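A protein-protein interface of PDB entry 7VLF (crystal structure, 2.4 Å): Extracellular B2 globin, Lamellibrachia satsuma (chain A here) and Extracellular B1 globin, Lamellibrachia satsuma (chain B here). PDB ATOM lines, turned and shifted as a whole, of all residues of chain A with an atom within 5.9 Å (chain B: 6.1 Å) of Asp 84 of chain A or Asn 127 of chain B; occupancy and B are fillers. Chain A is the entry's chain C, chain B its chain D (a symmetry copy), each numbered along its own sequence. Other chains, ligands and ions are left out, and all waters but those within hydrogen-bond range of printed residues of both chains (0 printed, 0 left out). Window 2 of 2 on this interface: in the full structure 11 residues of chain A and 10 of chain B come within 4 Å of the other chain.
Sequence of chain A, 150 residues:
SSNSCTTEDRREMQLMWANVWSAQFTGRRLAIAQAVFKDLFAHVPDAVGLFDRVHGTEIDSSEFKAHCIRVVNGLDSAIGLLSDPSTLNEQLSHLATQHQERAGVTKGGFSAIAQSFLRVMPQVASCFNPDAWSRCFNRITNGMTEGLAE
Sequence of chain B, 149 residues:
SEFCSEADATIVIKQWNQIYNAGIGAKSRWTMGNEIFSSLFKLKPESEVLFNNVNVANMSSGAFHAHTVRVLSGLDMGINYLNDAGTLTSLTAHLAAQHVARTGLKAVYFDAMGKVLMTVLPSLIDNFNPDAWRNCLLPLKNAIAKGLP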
ATOM      1  N   GLY A  80     -21.157 -32.110   5.610  1.00  0.00           N
ATOM      2  CA  GLY A  80     -21.518 -30.768   5.191  1.00  0.00           C
ATOM      3  C   GLY A  80     -21.900 -29.866   6.348  1.00  0.00           C
ATOM      4  O   GLY A  80     -21.630 -28.662   6.314  1.00  0.00           O
ATOM      5  N   LEU A  81     -22.517 -30.429   7.389  1.00  0.00           N
ATOM      6  CA  LEU A  81     -22.887 -29.661   8.571  1.00  0.00           C
ATOM      7  C   LEU A  81     -21.726 -29.449   9.533  1.00  0.00           C
ATOM      8  O   LEU A  81     -21.929 -28.848  10.594  1.00  0.00           O
ATOM      9  CB  LEU A  81     -24.040 -30.345   9.312  1.00  0.00           C
ATOM     10  CG  LEU A  81     -25.427 -30.192   8.691  1.00  0.00           C
ATOM     11  CD1 LEU A  81     -26.450 -31.016   9.455  1.00  0.00           C
ATOM     12  CD2 LEU A  81     -25.831 -28.728   8.658  1.00  0.00           C
ATOM     13  N   LEU A  82     -20.526 -29.927   9.199  1.00  0.00           N
ATOM     14  CA  LEU A  82     -19.365 -29.641  10.036  1.00  0.00           C
ATOM     15  C   LEU A  82     -19.059 -28.150  10.069  1.00  0.00           C
ATOM     16  O   LEU A  82     -18.469 -27.657  11.038  1.00  0.00           O
ATOM     17  CB  LEU A  82     -18.151 -30.425   9.537  1.00  0.00           C
ATOM     18  CG  LEU A  82     -18.124 -31.927   9.829  1.00  0.00           C
ATOM     19  CD1 LEU A  82     -16.963 -32.583   9.102  1.00  0.00           C
ATOM     20  CD2 LEU A  82     -18.021 -32.172  11.325  1.00  0.00           C
ATOM     21  N   SER A  83     -19.454 -27.417   9.025  1.00  0.00           N
ATOM     22  CA  SER A  83     -19.233 -25.975   9.000  1.00  0.00           C
ATOM     23  C   SER A  83     -20.158 -25.258   9.973  1.00  0.00           C
ATOM     24  O   SER A  83     -19.774 -24.248  10.577  1.00  0.00           O
ATOM     25  CB  SER A  83     -19.430 -25.442   7.583  1.00  0.00           C
ATOM     26  OG  SER A  83     -18.620 -26.143   6.653  1.00  0.00           O
ATOM     27  N   ASP A  84     -21.381 -25.763  10.140  1.00  0.00           N
ATOM     28  CA  ASP A  84     -22.373 -25.187  11.043  1.00  0.00           C
ATOM     29  C   ASP A  84     -22.616 -26.170  12.183  1.00  0.00           C
ATOM     30  O   ASP A  84     -23.542 -26.996  12.118  1.00  0.00           O
ATOM     31  CB  ASP A  84     -23.673 -24.888  10.294  1.00  0.00           C
ATOM     32  CG  ASP A  84     -23.571 -23.649   9.426  1.00  0.00           C
ATOM     33  OD1 ASP A  84     -23.445 -22.545   9.987  1.00  0.00           O
ATOM     34  OD2 ASP A  84     -23.618 -23.783   8.185  1.00  0.00           O
ATOM     35  N   PRO A  85     -21.823 -26.120  13.259  1.00  0.00           N
ATOM     36  CA  PRO A  85     -21.947 -27.149  14.304  1.00  0.00           C
ATOM     37  C   PRO A  85     -23.238 -27.064  15.093  1.00  0.00           C
ATOM     38  O   PRO A  85     -23.677 -28.088  15.633  1.00  0.00           O
ATOM     39  CB  PRO A  85     -20.722 -26.887  15.195  1.00  0.00           C
ATOM     40  CG  PRO A  85     -19.777 -26.102  14.340  1.00  0.00           C
ATOM     41  CD  PRO A  85     -20.657 -25.252  13.476  1.00  0.00           C
ATOM     42  N   SER A  86     -23.857 -25.887  15.184  1.00  0.00           N
ATOM     43  CA  SER A  86     -25.113 -25.768  15.918  1.00  0.00           C
ATOM     44  C   SER A  86     -26.199 -26.612  15.265  1.00  0.00           C
ATOM     45  O   SER A  86     -26.845 -27.438  15.920  1.00  0.00           O
ATOM     46  CB  SER A  86     -25.544 -24.302  15.998  1.00  0.00           C
ATOM     47  OG  SER A  86     -25.907 -23.807  14.721  1.00  0.00           O
ATOM     48  N   THR A  87     -26.417 -26.412  13.963  1.00  0.00           N
ATOM     49  CA  THR A  87     -27.331 -27.273  13.221  1.00  0.00           C
ATOM     50  C   THR A  87     -26.877 -28.726  13.259  1.00  0.00           C
ATOM     51  O   THR A  87     -27.710 -29.639  13.274  1.00  0.00           O
ATOM     52  CB  THR A  87     -27.442 -26.784  11.776  1.00  0.00           C
ATOM     53  OG1 THR A  87     -27.798 -25.396  11.764  1.00  0.00           O
ATOM     54  CG2 THR A  87     -28.495 -27.577  11.023  1.00  0.00           C
ATOM     55  N   LEU A  88     -25.564 -28.957  13.291  1.00  0.00           N
ATOM     56  CA  LEU A  88     -25.047 -30.318  13.364  1.00  0.00           C
ATOM     57  C   LEU A  88     -25.413 -30.977  14.688  1.00  0.00           C
ATOM     58  O   LEU A  88     -25.827 -32.142  14.717  1.00  0.00           O
ATOM     59  CB  LEU A  88     -23.533 -30.308  13.164  1.00  0.00           C
ATOM     60  CG  LEU A  88     -22.813 -31.655  13.207  1.00  0.00           C
ATOM     61  CD1 LEU A  88     -23.364 -32.597  12.150  1.00  0.00           C
ATOM     62  CD2 LEU A  88     -21.319 -31.454  13.023  1.00  0.00           C
ATOM     63  N   ASN A  89     -25.270 -30.248  15.798  1.00  0.00           N
ATOM     64  CA  ASN A  89     -25.624 -30.813  17.097  1.00  0.00           C
ATOM     65  C   ASN A  89     -27.107 -31.136  17.174  1.00  0.00           C
ATOM     66  O   ASN A  89     -27.494 -32.198  17.677  1.00  0.00           O
ATOM     67  CB  ASN A  89     -25.235 -29.855  18.220  1.00  0.00           C
ATOM     68  CG  ASN A  89     -23.782 -29.978  18.604  1.00  0.00           C
ATOM     69  OD1 ASN A  89     -23.191 -31.054  18.504  1.00  0.00           O
ATOM     70  ND2 ASN A  89     -23.194 -28.876  19.047  1.00  0.00           N
ATOM     71  N   GLN B  15     -15.033 -14.507  17.761  1.00  0.00           N
ATOM     72  CA  GLN B  15     -16.401 -14.450  18.267  1.00  0.00           C
ATOM     73  C   GLN B  15     -16.448 -13.981  19.716  1.00  0.00           C
ATOM     74  O   GLN B  15     -17.453 -13.407  20.147  1.00  0.00           O
ATOM     75  CB  GLN B  15     -17.074 -15.814  18.118  1.00  0.00           C
ATOM     76  CG  GLN B  15     -17.234 -16.257  16.668  1.00  0.00           C
ATOM     77  CD  GLN B  15     -17.948 -17.586  16.530  1.00  0.00           C
ATOM     78  OE1 GLN B  15     -18.385 -17.960  15.441  1.00  0.00           O
ATOM     79  NE2 GLN B  15     -18.068 -18.311  17.634  1.00  0.00           N
ATOM     80  N   ILE B 125     -23.780 -14.246  20.639  1.00  0.00           N
ATOM     81  CA  ILE B 125     -22.822 -14.283  19.539  1.00  0.00           C
ATOM     82  C   ILE B 125     -23.523 -14.755  18.275  1.00  0.00           C
ATOM     83  O   ILE B 125     -24.345 -15.680  18.311  1.00  0.00           O
ATOM     84  CB  ILE B 125     -21.625 -15.193  19.881  1.00  0.00           C
ATOM     85  CG1 ILE B 125     -20.944 -14.713  21.164  1.00  0.00           C
ATOM     86  CG2 ILE B 125     -20.626 -15.230  18.732  1.00  0.00           C
ATOM     87  CD1 ILE B 125     -19.696 -15.493  21.525  1.00  0.00           C
ATOM     88  N   ASP B 126     -23.201 -14.115  17.152  1.00  0.00           N
ATOM     89  CA  ASP B 126     -23.742 -14.509  15.859  1.00  0.00           C
ATOM     90  C   ASP B 126     -23.026 -15.752  15.353  1.00  0.00           C
ATOM     91  O   ASP B 126     -21.792 -15.791  15.302  1.00  0.00           O
ATOM     92  CB  ASP B 126     -23.591 -13.372  14.851  1.00  0.00           C
ATOM     93  CG  ASP B 126     -24.213 -12.084  15.335  1.00  0.00           C
ATOM     94  OD1 ASP B 126     -24.819 -12.092  16.426  1.00  0.00           O
ATOM     95  OD2 ASP B 126     -24.088 -11.059  14.631  1.00  0.00           O
ATOM     96  N   ASN B 127     -23.805 -16.762  14.970  1.00  0.00           N
ATOM     97  CA  ASN B 127     -23.286 -18.025  14.447  1.00  0.00           C
ATOM     98  C   ASN B 127     -22.263 -18.636  15.404  1.00  0.00           C
ATOM     99  O   ASN B 127     -21.104 -18.879  15.061  1.00  0.00           O
ATOM    100  CB  ASN B 127     -22.695 -17.838  13.049  1.00  0.00           C
ATOM    101  CG  ASN B 127     -23.538 -18.489  11.971  1.00  0.00           C
ATOM    102  OD1 ASN B 127     -23.992 -19.623  12.124  1.00  0.00           O
ATOM    103  ND2 ASN B 127     -23.760 -17.769  10.880  1.00  0.00           N
ATOM    104  N   PHE B 128     -22.723 -18.876  16.630  1.00  0.00           N
ATOM    105  CA  PHE B 128     -21.892 -19.519  17.638  1.00  0.00           C
ATOM    106  C   PHE B 128     -21.472 -20.908  17.173  1.00  0.00           C
ATOM    107  O   PHE B 128     -22.280 -21.678  16.647  1.00  0.00           O
ATOM    108  CB  PHE B 128     -22.659 -19.599  18.961  1.00  0.00           C
ATOM    109  CG  PHE B 128     -21.952 -20.372  20.036  1.00  0.00           C
ATOM    110  CD1 PHE B 128     -20.914 -19.804  20.752  1.00  0.00           C
ATOM    111  CD2 PHE B 128     -22.346 -21.662  20.350  1.00  0.00           C
ATOM    112  CE1 PHE B 128     -20.270 -20.513  21.749  1.00  0.00           C
ATOM    113  CE2 PHE B 128     -21.707 -22.376  21.346  1.00  0.00           C
ATOM    114  CZ  PHE B 128     -20.668 -21.801  22.046  1.00  0.00           C
ATOM    115  N   ASN B 129     -20.188 -21.219  17.358  1.00  0.00           N
ATOM    116  CA  ASN B 129     -19.598 -22.482  16.920  1.00  0.00           C
ATOM    117  C   ASN B 129     -19.341 -23.364  18.135  1.00  0.00           C
ATOM    118  O   ASN B 129     -18.277 -23.270  18.762  1.00  0.00           O
ATOM    119  CB  ASN B 129     -18.303 -22.228  16.144  1.00  0.00           C
ATOM    120  CG  ASN B 129     -17.781 -23.470  15.449  1.00  0.00           C
ATOM    121  OD1 ASN B 129     -17.604 -24.520  16.068  1.00  0.00           O
ATOM    122  ND2 ASN B 129     -17.535 -23.356  14.149  1.00  0.00           N
ATOM    123  N   PRO B 130     -20.275 -24.246  18.502  1.00  0.00           N
ATOM    124  CA  PRO B 130     -20.072 -25.052  19.719  1.00  0.00           C
ATOM    125  C   PRO B 130     -18.860 -25.962  19.653  1.00  0.00           C
ATOM    126  O   PRO B 130     -18.193 -26.167  20.673  1.00  0.00           O
ATOM    127  CB  PRO B 130     -21.381 -25.851  19.829  1.00  0.00           C
ATOM    128  CG  PRO B 130     -21.944 -25.861  18.448  1.00  0.00           C
ATOM    129  CD  PRO B 130     -21.556 -24.548  17.843  1.00  0.00           C
ATOM    130  N   ASP B 131     -18.551 -26.509  18.477  1.00  0.00           N
ATOM    131  CA  ASP B 131     -17.421 -27.423  18.355  1.00  0.00           C
ATOM    132  C   ASP B 131     -16.103 -26.711  18.637  1.00  0.00           C
ATOM    133  O   ASP B 131     -15.328 -27.131  19.503  1.00  0.00           O
ATOM    134  CB  ASP B 131     -17.410 -28.050  16.962  1.00  0.00           C
ATOM    135  CG  ASP B 131     -18.405 -29.176  16.825  1.00  0.00           C
ATOM    136  OD1 ASP B 131     -18.689 -29.837  17.846  1.00  0.00           O
ATOM    137  OD2 ASP B 131     -18.899 -29.405  15.700  1.00  0.00           O
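The backbone carbonyl oxygen of Asn 127 of chain B lies close to the side-chain amide oxygen of Gln 15 of chain B (2.9 Å). The side-chain amide oxygen of Asn 129 of chain B sits close to the backbone NH of Asp 131 of chain B.
Of the 8 printed residues of chain B, 4 touch a printed residue of chain A. Hydrophobic or aromatic side chains of chain B within 4 Å of the printed part of chain A: Pro 130. Among the printed residues, no Asp or Glu carboxylate lies within 4 Å of a Lys or Arg side-chain nitrogen of the other chain.
Asp 84 of chain A touches one residue of chain B. Of the printed residues of chain B, Ser 86 of chain A touches Pro 130. Thr 87 of chain A touches none of the printed residues of chain B. Printed residues of chain B within 4 Å of Asn 89 of chain A: Pro 130 (3.3 Å). Ile 125 of chain B touches none of the printed residues of chain A. Asn 127 of chain B touches one residue of chain A. Of the printed residues of chain A, Asn 129 of chain B touches Pro 85 (3.2 Å). Printed residues of chain A within 4 Å of Asp 131 of chain B: Pro 85. The nearest residue of chain A that does not touch Asn 127 of chain B is Ser 86 of chain A (5.3 Å).
OD1 of Asp 84 of chain A touches OD1 of Asn 127 of chain B (3.7 Å). Pro 85 of chain A touches Asn 129 of chain B. Pro 130 of chain B touches Pro 85 of chain A. Pro 85 of chain A touches Asp 131 of chain B. Ser 86 of chain A touches Pro 130 of chain B. Asn 89 of chain A touches Pro 130 of chain B (ND2 to CG, 3.3 Å).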
